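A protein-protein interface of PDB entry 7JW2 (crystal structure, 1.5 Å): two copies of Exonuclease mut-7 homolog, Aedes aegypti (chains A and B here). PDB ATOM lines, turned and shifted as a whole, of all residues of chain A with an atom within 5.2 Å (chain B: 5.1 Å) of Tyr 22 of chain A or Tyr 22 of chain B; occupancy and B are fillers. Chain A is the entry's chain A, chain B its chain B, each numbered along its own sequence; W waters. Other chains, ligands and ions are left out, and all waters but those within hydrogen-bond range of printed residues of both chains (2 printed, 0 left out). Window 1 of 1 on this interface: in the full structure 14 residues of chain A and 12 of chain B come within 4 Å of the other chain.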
ATOM      1  N   LYS A  18      19.073  13.803  -7.513  1.00  0.00           N
ATOM      2  CA  LYS A  18      18.138  12.702  -7.315  1.00  0.00           C
ATOM      3  C   LYS A  18      17.115  12.648  -8.434  1.00  0.00           C
ATOM      4  O   LYS A  18      16.765  11.553  -8.892  1.00  0.00           O
ATOM      5  CB  LYS A  18      17.469  12.804  -5.939  1.00  0.00           C
ATOM      6  CG  LYS A  18      17.901  11.626  -5.059  1.00  0.00           C
ATOM      7  CD  LYS A  18      17.709  11.809  -3.559  1.00  0.00           C
ATOM      8  CE  LYS A  18      18.930  11.243  -2.839  1.00  0.00           C
ATOM      9  NZ  LYS A  18      18.628  10.455  -1.629  1.00  0.00           N
ATOM     10  N   ASP A  19      16.653  13.800  -8.932  1.00  0.00           N
ATOM     11  CA  ASP A  19      15.719  13.781 -10.055  1.00  0.00           C
ATOM     12  C   ASP A  19      16.344  13.140 -11.282  1.00  0.00           C
ATOM     13  O   ASP A  19      15.676  12.394 -11.998  1.00  0.00           O
ATOM     14  CB  ASP A  19      15.225  15.190 -10.386  1.00  0.00           C
ATOM     15  CG  ASP A  19      16.342  16.189 -10.647  1.00  0.00           C
ATOM     16  OD1 ASP A  19      16.442  16.702 -11.777  1.00  0.00           O
ATOM     17  OD2 ASP A  19      17.104  16.453  -9.720  1.00  0.00           O
ATOM     18  N   LYS A  20      17.626  13.398 -11.537  1.00  0.00           N
ATOM     19  CA  LYS A  20      18.284  12.806 -12.696  1.00  0.00           C
ATOM     20  C   LYS A  20      18.479  11.307 -12.515  1.00  0.00           C
ATOM     21  O   LYS A  20      18.385  10.553 -13.489  1.00  0.00           O
ATOM     22  CB  LYS A  20      19.629  13.503 -12.953  1.00  0.00           C
ATOM     23  CG  LYS A  20      19.467  14.925 -13.461  1.00  0.00           C
ATOM     24  CD  LYS A  20      20.798  15.653 -13.560  1.00  0.00           C
ATOM     25  CE  LYS A  20      20.567  17.144 -13.787  1.00  0.00           C
ATOM     26  NZ  LYS A  20      21.821  17.912 -13.578  1.00  0.00           N
ATOM     27  N   PHE A  21      18.733  10.869 -11.281  1.00  0.00           N
ATOM     28  CA  PHE A  21      18.878   9.445 -10.988  1.00  0.00           C
ATOM     29  C   PHE A  21      17.582   8.684 -11.275  1.00  0.00           C
ATOM     30  O   PHE A  21      17.594   7.614 -11.907  1.00  0.00           O
ATOM     31  CB  PHE A  21      19.305   9.289  -9.530  1.00  0.00           C
ATOM     32  CG  PHE A  21      19.514   7.876  -9.091  1.00  0.00           C
ATOM     33  CD1 PHE A  21      18.508   7.196  -8.427  1.00  0.00           C
ATOM     34  CD2 PHE A  21      20.727   7.239  -9.296  1.00  0.00           C
ATOM     35  CE1 PHE A  21      18.701   5.894  -8.002  1.00  0.00           C
ATOM     36  CE2 PHE A  21      20.920   5.934  -8.869  1.00  0.00           C
ATOM     37  CZ  PHE A  21      19.910   5.269  -8.225  1.00  0.00           C
ATOM     38  N   TYR A  22      16.443   9.227 -10.841  1.00  0.00           N
ATOM     39  CA  TYR A  22      15.179   8.527 -11.078  1.00  0.00           C
ATOM     40  C   TYR A  22      14.753   8.622 -12.536  1.00  0.00           C
ATOM     41  O   TYR A  22      14.104   7.701 -13.042  1.00  0.00           O
ATOM     42  CB  TYR A  22      14.097   9.052 -10.122  1.00  0.00           C
ATOM     43  CG  TYR A  22      14.318   8.467  -8.748  1.00  0.00           C
ATOM     44  CD1 TYR A  22      14.107   7.117  -8.518  1.00  0.00           C
ATOM     45  CD2 TYR A  22      14.785   9.237  -7.702  1.00  0.00           C
ATOM     46  CE1 TYR A  22      14.333   6.550  -7.277  1.00  0.00           C
ATOM     47  CE2 TYR A  22      15.008   8.681  -6.449  1.00  0.00           C
ATOM     48  CZ  TYR A  22      14.791   7.338  -6.248  1.00  0.00           C
ATOM     49  OH  TYR A  22      15.022   6.778  -5.012  1.00  0.00           O
ATOM     50  N   ALA A  23      15.113   9.700 -13.241  1.00  0.00           N
ATOM     51  CA  ALA A  23      14.856   9.739 -14.679  1.00  0.00           C
ATOM     52  C   ALA A  23      15.667   8.669 -15.400  1.00  0.00           C
ATOM     53  O   ALA A  23      15.160   7.986 -16.309  1.00  0.00           O
ATOM     54  CB  ALA A  23      15.177  11.127 -15.238  1.00  0.00           C
ATOM     55  N   MET A  24      16.922   8.485 -14.988  1.00  0.00           N
ATOM     56  CA  MET A  24      17.736   7.388 -15.512  1.00  0.00           C
ATOM     57  C   MET A  24      17.089   6.037 -15.224  1.00  0.00           C
ATOM     58  O   MET A  24      16.984   5.179 -16.113  1.00  0.00           O
ATOM     59  CB  MET A  24      19.140   7.456 -14.903  1.00  0.00           C
ATOM     60  CG  MET A  24      19.977   6.215 -15.195  1.00  0.00           C
ATOM     61  SD  MET A  24      21.465   6.186 -14.161  1.00  0.00           S
ATOM     62  CE  MET A  24      20.744   5.618 -12.603  1.00  0.00           C
ATOM     63  N   LEU A  25      16.668   5.815 -13.975  1.00  0.00           N
ATOM     64  CA  LEU A  25      16.065   4.538 -13.605  1.00  0.00           C
ATOM     65  C   LEU A  25      14.821   4.266 -14.435  1.00  0.00           C
ATOM     66  O   LEU A  25      14.560   3.127 -14.832  1.00  0.00           O
ATOM     67  CB  LEU A  25      15.724   4.516 -12.113  1.00  0.00           C
ATOM     68  CG  LEU A  25      15.464   3.125 -11.524  1.00  0.00           C
ATOM     69  CD1 LEU A  25      16.727   2.272 -11.688  1.00  0.00           C
ATOM     70  CD2 LEU A  25      15.086   3.212 -10.052  1.00  0.00           C
ATOM     71  N   SER A  26      14.042   5.308 -14.720  1.00  0.00           N
ATOM     72  CA  SER A  26      12.845   5.150 -15.540  1.00  0.00           C
ATOM     73  C   SER A  26      13.176   4.556 -16.904  1.00  0.00           C
ATOM     74  O   SER A  26      12.457   3.677 -17.398  1.00  0.00           O
ATOM     75  CB  SER A  26      12.154   6.502 -15.701  1.00  0.00           C
ATOM     76  OG  SER A  26      11.078   6.413 -16.615  1.00  0.00           O
ATOM     77  N   CYS A  29      15.037   0.689 -16.355  1.00  0.00           N
ATOM     78  CA  CYS A  29      14.245  -0.438 -15.880  1.00  0.00           C
ATOM     79  C   CYS A  29      13.442  -1.107 -16.988  1.00  0.00           C
ATOM     80  O   CYS A  29      12.936  -2.208 -16.765  1.00  0.00           O
ATOM     81  CB  CYS A  29      13.322  -0.007 -14.741  1.00  0.00           C
ATOM     82  SG  CYS A  29      11.879   0.919 -15.249  1.00  0.00           S
ATOM     83  N   LEU A  74      18.494   3.533  -0.076  1.00  0.00           N
ATOM     84  CA  LEU A  74      17.314   3.232  -0.888  1.00  0.00           C
ATOM     85  C   LEU A  74      17.601   3.431  -2.372  1.00  0.00           C
ATOM     86  O   LEU A  74      17.132   2.650  -3.208  1.00  0.00           O
ATOM     87  CB  LEU A  74      16.137   4.108  -0.443  1.00  0.00           C
ATOM     88  CG  LEU A  74      14.793   4.071  -1.192  1.00  0.00           C
ATOM     89  CD1 LEU A  74      14.779   4.894  -2.480  1.00  0.00           C
ATOM     90  CD2 LEU A  74      14.370   2.661  -1.454  1.00  0.00           C
ATOM     91  N   ASP A  75      18.347   4.483  -2.722  1.00  0.00           N
ATOM     92  CA  ASP A  75      18.623   4.758  -4.130  1.00  0.00           C
ATOM     93  C   ASP A  75      19.481   3.657  -4.742  1.00  0.00           C
ATOM     94  O   ASP A  75      19.180   3.148  -5.839  1.00  0.00           O
ATOM     95  CB  ASP A  75      19.314   6.125  -4.268  1.00  0.00           C
ATOM     96  CG  ASP A  75      18.513   7.250  -3.635  1.00  0.00           C
ATOM     97  OD1 ASP A  75      17.294   7.368  -3.884  1.00  0.00           O
ATOM     98  OD2 ASP A  75      19.105   8.049  -2.870  1.00  0.00           O
ATOM     99  N   ALA A  78      17.549   0.512  -5.151  1.00  0.00           N
ATOM    100  CA  ALA A  78      16.630   0.566  -6.283  1.00  0.00           C
ATOM    101  C   ALA A  78      17.361   0.298  -7.593  1.00  0.00           C
ATOM    102  O   ALA A  78      16.818  -0.364  -8.486  1.00  0.00           O
ATOM    103  CB  ALA A  78      15.924   1.918  -6.335  1.00  0.00           C
ATOM    104  N   ASN A  82      16.377  -3.019  -9.827  1.00  0.00           N
ATOM    105  CA  ASN A  82      15.649  -2.792 -11.068  1.00  0.00           C
ATOM    106  C   ASN A  82      16.532  -2.855 -12.304  1.00  0.00           C
ATOM    107  O   ASN A  82      16.001  -2.792 -13.427  1.00  0.00           O
ATOM    108  CB  ASN A  82      14.905  -1.463 -11.000  1.00  0.00           C
ATOM    109  CG  ASN A  82      13.745  -1.523 -10.041  1.00  0.00           C
ATOM    110  OD1 ASN A  82      12.733  -2.165 -10.324  1.00  0.00           O
ATOM    111  ND2 ASN A  82      13.887  -0.885  -8.881  1.00  0.00           N
ATOM    112  N   LYS B  18       6.352   0.468 -13.864  1.00  0.00           N
ATOM    113  CA  LYS B  18       7.499   0.915 -13.076  1.00  0.00           C
ATOM    114  C   LYS B  18       8.219   2.087 -13.734  1.00  0.00           C
ATOM    115  O   LYS B  18       8.649   3.017 -13.038  1.00  0.00           O
ATOM    116  CB  LYS B  18       8.479  -0.237 -12.854  1.00  0.00           C
ATOM    117  CG  LYS B  18       8.118  -1.162 -11.715  1.00  0.00           C
ATOM    118  CD  LYS B  18       9.201  -2.226 -11.539  1.00  0.00           C
ATOM    119  CE  LYS B  18       9.033  -2.970 -10.233  1.00  0.00           C
ATOM    120  NZ  LYS B  18      10.113  -2.672  -9.233  1.00  0.00           N
ATOM    121  N   ASP B  19       8.368   2.077 -15.060  1.00  0.00           N
ATOM    122  CA  ASP B  19       9.074   3.186 -15.696  1.00  0.00           C
ATOM    123  C   ASP B  19       8.306   4.495 -15.531  1.00  0.00           C
ATOM    124  O   ASP B  19       8.911   5.544 -15.291  1.00  0.00           O
ATOM    125  CB  ASP B  19       9.355   2.898 -17.171  1.00  0.00           C
ATOM    126  CG  ASP B  19       8.112   2.585 -17.955  1.00  0.00           C
ATOM    127  OD1 ASP B  19       7.755   3.392 -18.836  1.00  0.00           O
ATOM    128  OD2 ASP B  19       7.515   1.528 -17.701  1.00  0.00           O
ATOM    129  N   LYS B  20       6.975   4.453 -15.627  1.00  0.00           N
ATOM    130  CA  LYS B  20       6.201   5.672 -15.435  1.00  0.00           C
ATOM    131  C   LYS B  20       6.243   6.103 -13.986  1.00  0.00           C
ATOM    132  O   LYS B  20       6.232   7.304 -13.697  1.00  0.00           O
ATOM    133  CB  LYS B  20       4.758   5.469 -15.898  1.00  0.00           C
ATOM    134  CG  LYS B  20       4.659   5.198 -17.402  1.00  0.00           C
ATOM    135  CD  LYS B  20       3.217   4.871 -17.814  1.00  0.00           C
ATOM    136  CE  LYS B  20       3.127   4.520 -19.300  1.00  0.00           C
ATOM    137  NZ  LYS B  20       1.851   3.831 -19.632  1.00  0.00           N
ATOM    138  N   PHE B  21       6.318   5.140 -13.069  1.00  0.00           N
ATOM    139  CA  PHE B  21       6.444   5.458 -11.652  1.00  0.00           C
ATOM    140  C   PHE B  21       7.748   6.203 -11.358  1.00  0.00           C
ATOM    141  O   PHE B  21       7.753   7.202 -10.621  1.00  0.00           O
ATOM    142  CB  PHE B  21       6.329   4.160 -10.840  1.00  0.00           C
ATOM    143  CG  PHE B  21       6.504   4.338  -9.359  1.00  0.00           C
ATOM    144  CD1 PHE B  21       7.736   4.078  -8.766  1.00  0.00           C
ATOM    145  CD2 PHE B  21       5.456   4.757  -8.557  1.00  0.00           C
ATOM    146  CE1 PHE B  21       7.909   4.223  -7.408  1.00  0.00           C
ATOM    147  CE2 PHE B  21       5.637   4.915  -7.184  1.00  0.00           C
ATOM    148  CZ  PHE B  21       6.873   4.643  -6.618  1.00  0.00           C
ATOM    149  N   TYR B  22       8.860   5.744 -11.931  1.00  0.00           N
ATOM    150  CA  TYR B  22      10.122   6.420 -11.654  1.00  0.00           C
ATOM    151  C   TYR B  22      10.206   7.761 -12.366  1.00  0.00           C
ATOM    152  O   TYR B  22      10.849   8.684 -11.847  1.00  0.00           O
ATOM    153  CB  TYR B  22      11.297   5.485 -11.986  1.00  0.00           C
ATOM    154  CG  TYR B  22      11.443   4.516 -10.836  1.00  0.00           C
ATOM    155  CD1 TYR B  22      11.873   4.978  -9.598  1.00  0.00           C
ATOM    156  CD2 TYR B  22      11.038   3.198 -10.930  1.00  0.00           C
ATOM    157  CE1 TYR B  22      11.974   4.136  -8.504  1.00  0.00           C
ATOM    158  CE2 TYR B  22      11.122   2.338  -9.824  1.00  0.00           C
ATOM    159  CZ  TYR B  22      11.592   2.822  -8.620  1.00  0.00           C
ATOM    160  OH  TYR B  22      11.698   2.010  -7.506  1.00  0.00           O
ATOM    161  N   ALA B  23       9.549   7.913 -13.518  1.00  0.00           N
ATOM    162  CA  ALA B  23       9.486   9.221 -14.160  1.00  0.00           C
ATOM    163  C   ALA B  23       8.709  10.199 -13.289  1.00  0.00           C
ATOM    164  O   ALA B  23       9.117  11.360 -13.116  1.00  0.00           O
ATOM    165  CB  ALA B  23       8.848   9.101 -15.546  1.00  0.00           C
ATOM    166  N   MET B  24       7.601   9.736 -12.708  1.00  0.00           N
ATOM    167  CA  MET B  24       6.871  10.557 -11.748  1.00  0.00           C
ATOM    168  C   MET B  24       7.763  10.959 -10.573  1.00  0.00           C
ATOM    169  O   MET B  24       7.785  12.130 -10.163  1.00  0.00           O
ATOM    170  CB  MET B  24       5.639   9.797 -11.258  1.00  0.00           C
ATOM    171  CG  MET B  24       4.961  10.423 -10.031  1.00  0.00           C
ATOM    172  SD  MET B  24       3.733   9.315  -9.310  1.00  0.00           S
ATOM    173  CE  MET B  24       4.793   8.259  -8.356  1.00  0.00           C
ATOM    174  N   LEU B  25       8.487   9.994  -9.990  1.00  0.00           N
ATOM    175  CA  LEU B  25       9.337  10.312  -8.848  1.00  0.00           C
ATOM    176  C   LEU B  25      10.411  11.318  -9.222  1.00  0.00           C
ATOM    177  O   LEU B  25      10.784  12.156  -8.392  1.00  0.00           O
ATOM    178  CB  LEU B  25       9.997   9.056  -8.281  1.00  0.00           C
ATOM    179  CG  LEU B  25       9.127   8.147  -7.418  1.00  0.00           C
ATOM    180  CD1 LEU B  25       9.947   6.998  -6.847  1.00  0.00           C
ATOM    181  CD2 LEU B  25       8.439   8.923  -6.304  1.00  0.00           C
ATOM    182  N   SER B  26      10.913  11.268 -10.459  1.00  0.00           N
ATOM    183  CA  SER B  26      11.908  12.237 -10.899  1.00  0.00           C
ATOM    184  C   SER B  26      11.378  13.659 -10.754  1.00  0.00           C
ATOM    185  O   SER B  26      12.089  14.551 -10.273  1.00  0.00           O
ATOM    186  CB  SER B  26      12.303  11.941 -12.346  1.00  0.00           C
ATOM    187  OG  SER B  26      13.165  12.936 -12.858  1.00  0.00           O
ATOM    188  N   CYS B  29      10.297  14.384  -6.597  1.00  0.00           N
ATOM    189  CA  CYS B  29      11.333  14.496  -5.586  1.00  0.00           C
ATOM    190  C   CYS B  29      11.957  15.888  -5.548  1.00  0.00           C
ATOM    191  O   CYS B  29      12.669  16.191  -4.584  1.00  0.00           O
ATOM    192  CB  CYS B  29      12.401  13.418  -5.800  1.00  0.00           C
ATOM    193  SG  CYS B  29      13.541  13.772  -7.129  1.00  0.00           S
ATOM    194  N   LEU B  74       9.892  -2.109  -2.501  1.00  0.00           N
ATOM    195  CA  LEU B  74      10.904  -1.060  -2.557  1.00  0.00           C
ATOM    196  C   LEU B  74      10.415   0.161  -3.330  1.00  0.00           C
ATOM    197  O   LEU B  74      10.841   1.289  -3.041  1.00  0.00           O
ATOM    198  CB  LEU B  74      12.189  -1.609  -3.174  1.00  0.00           C
ATOM    199  CG  LEU B  74      13.447  -0.782  -2.915  1.00  0.00           C
ATOM    200  CD1 LEU B  74      13.795  -0.741  -1.416  1.00  0.00           C
ATOM    201  CD2 LEU B  74      14.594  -1.361  -3.710  1.00  0.00           C
ATOM    202  N   ASP B  75       9.525  -0.036  -4.306  1.00  0.00           N
ATOM    203  CA  ASP B  75       8.945   1.108  -5.008  1.00  0.00           C
ATOM    204  C   ASP B  75       8.096   1.949  -4.074  1.00  0.00           C
ATOM    205  O   ASP B  75       8.175   3.182  -4.094  1.00  0.00           O
ATOM    206  CB  ASP B  75       8.110   0.637  -6.199  1.00  0.00           C
ATOM    207  CG  ASP B  75       8.913  -0.196  -7.165  1.00  0.00           C
ATOM    208  OD1 ASP B  75      10.096   0.146  -7.423  1.00  0.00           O
ATOM    209  OD2 ASP B  75       8.378  -1.210  -7.665  1.00  0.00           O
ATOM    210  N   ALA B  78      10.252   3.919  -1.910  1.00  0.00           N
ATOM    211  CA  ALA B  78      10.821   5.065  -2.609  1.00  0.00           C
ATOM    212  C   ALA B  78       9.846   6.229  -2.633  1.00  0.00           C
ATOM    213  O   ALA B  78      10.257   7.388  -2.520  1.00  0.00           O
ATOM    214  CB  ALA B  78      11.209   4.670  -4.031  1.00  0.00           C
ATOM    215  N   ASN B  82      10.836   9.679  -0.792  1.00  0.00           N
ATOM    216  CA  ASN B  82      11.043  10.842  -1.654  1.00  0.00           C
ATOM    217  C   ASN B  82       9.902  11.848  -1.634  1.00  0.00           C
ATOM    218  O   ASN B  82      10.074  12.948  -2.177  1.00  0.00           O
ATOM    219  CB  ASN B  82      11.271  10.401  -3.101  1.00  0.00           C
ATOM    220  CG  ASN B  82      12.621   9.758  -3.303  1.00  0.00           C
ATOM    221  OD1 ASN B  82      13.657  10.422  -3.226  1.00  0.00           O
ATOM    222  ND2 ASN B  82      12.622   8.457  -3.576  1.00  0.00           N
HETATM  223  O   HOH W   1      12.046  -1.645  -6.784  1.00  0.00           O
HETATM  224  O   HOH W   2      15.895   9.088  -2.259  1.00  0.00           O
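The side-chain sulfur (SG) of Cys 29 of chain B sits at hydrogen-bond distance from the backbone NH (N) of Asp 19 of chain A (3.6 Å).
The backbone NH (N) of Asp 19 of chain B lies close to the side-chain sulfur (SG) of Cys 29 of chain A (3.7 Å).
OG of Ser 26 of chain A sits at hydrogen-bond distance from O of Asp 19 of chain B, 2.7 Å away.
The side-chain amide oxygen of Asn 82 of chain A is in hydrogen-bond range of the side-chain amino group of Lys 18 of chain B.
O of Asp 19 of chain A is in hydrogen-bond range of OG of Ser 26 of chain B (2.7 Å).
The side-chain amide nitrogen of Asn 82 of chain B sits at hydrogen-bond distance from the side-chain hydroxyl of Tyr 22 of chain A.
O of Ser 26 of chain B is in hydrogen-bond range of SG of Cys 29 of chain B, 3.5 Å away.
O of Ser 26 of chain A is in hydrogen-bond range of SG of Cys 29 of chain A (3.5 Å).
OD2 of Asp 75 of chain B is in salt-bridge range of NZ of Lys 18 of chain B, 2.8 Å away.
The backbone carbonyl oxygen of Ala 78 of chain B is in hydrogen-bond range of the side-chain amide nitrogen of Asn 82 of chain B, 2.8 Å away.
The side-chain carboxylate (OD1) of Asp 75 of chain B lies within hydrogen-bond range of the side-chain hydroxyl (OH) of Tyr 22 of chain B, 2.5 Å away.
OD1 of Asp 75 of chain A sits at hydrogen-bond distance from OH of Tyr 22 of chain A, at 2.6 Å.
Among the printed residues, pairs that only touch across the chains: Tyr 22 of chain A with Tyr 22 of chain B (3.3 Å), Leu 74 of chain A with Leu 74 of chain B (3.5 Å), Leu 25 of chain A with Tyr 22 of chain B (3.6 Å), Ala 23 of chain A with Ser 26 of chain B (3.6 Å), Ser 26 of chain A with Ala 23 of chain B (3.7 Å), Ala 78 of chain A with Leu 74 of chain B (3.8 Å), Ser 26 of chain A with Tyr 22 of chain B (3.9 Å), Asn 82 of chain A with Tyr 22 of chain B (3.9 Å), Tyr 22 of chain A with Ser 26 of chain B (3.9 Å), Leu 74 of chain A with Ala 78 of chain B (3.9 Å) and Lys 18 of chain A with Cys 29 of chain B (3.97 Å).
Of chain B, only Tyr 22 (3.3 Å), Ser 26 (3.9 Å) and Asn 82 (3.3 Å) come within 4 Å of Tyr 22 of chain A.
Of chain A, only Tyr 22 (3.3 Å), Leu 25 (3.6 Å), Ser 26 (3.9 Å) and Asn 82 (3.9 Å) come within 4 Å of Tyr 22 of chain B.
Printed residues of chain B within 4 Å of Asp 19 of chain A: Ser 26 (2.7 Å) and Cys 29 (3.6 Å).
Printed residues of chain A within 4 Å of Ser 26 of chain B: Asp 19, Tyr 22 and Ala 23.
Of the printed residues of chain B, Leu 74 of chain A touches Leu 74 (3.5 Å) and Ala 78 (3.9 Å).
Printed residues of chain A within 4 Å of Asp 19 of chain B: Ser 26 (2.7 Å) and Cys 29 (3.6 Å).
Phe 21 of chain B touches none of the printed residues of chain A.
Leu 25 of chain B touches none of the printed residues of chain A.
The nearest residue of chain B that does not touch Tyr 22 of chain A is Leu 25 of chain B (4.4 Å).
The nearest printed residue of chain A that does not touch Cys 29 of chain B is Tyr 22 of chain A (4.7 Å).
Hydrophobic or aromatic side chains of chain B within 4 Å of the printed part of chain A: Tyr 22, Ala 23, Leu 74 and Ala 78.
Among the printed residues, 17 pairs touch across the chains.
Among the printed residues, no Asp or Glu carboxylate lies within 4 Å of a Lys or Arg side-chain nitrogen of the other chain.
Asp 19 of chain A touches Cys 29 of chain B, and with the chains exchanged Cys 29 of chain A touches Asp 19 of chain B.
Tyr 22 of chain A touches Ser 26 of chain B, and with the chains exchanged Ser 26 of chain A touches Tyr 22 of chain B.
Leu 25 of chain A touches Tyr 22 of chain B, but with the chains exchanged Tyr 22 of chain A does not touch Leu 25 of chain B (4.4 Å).
Asn 82 of chain A touches Lys 18 of chain B, but with the chains exchanged Lys 18 of chain A does not touch Asn 82 of chain B (4.3 Å).
Positions printed for both chains: 18, 19, 20, 21, 22, 23, 24, 25, 26, 29, 74, 75, 78 and 82.
Of the 17 pairs that touch across the chains among the printed residues, 14 have their exchanged pair printed and touching as well.
Water W1 lies within hydrogen-bond range of OD1 of Asp 75 of chain B (2.7 Å), ND2 of Asn 82 of chain A (2.9 Å) and NZ of Lys 18 of chain B (3.3 Å).
Water W2 lies within hydrogen-bond range of the side-chain carboxylate of Asp 75 of chain A, the side-chain amide oxygen of Asn 82 of chain B and the side-chain amino group of Lys 18 of chain A.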
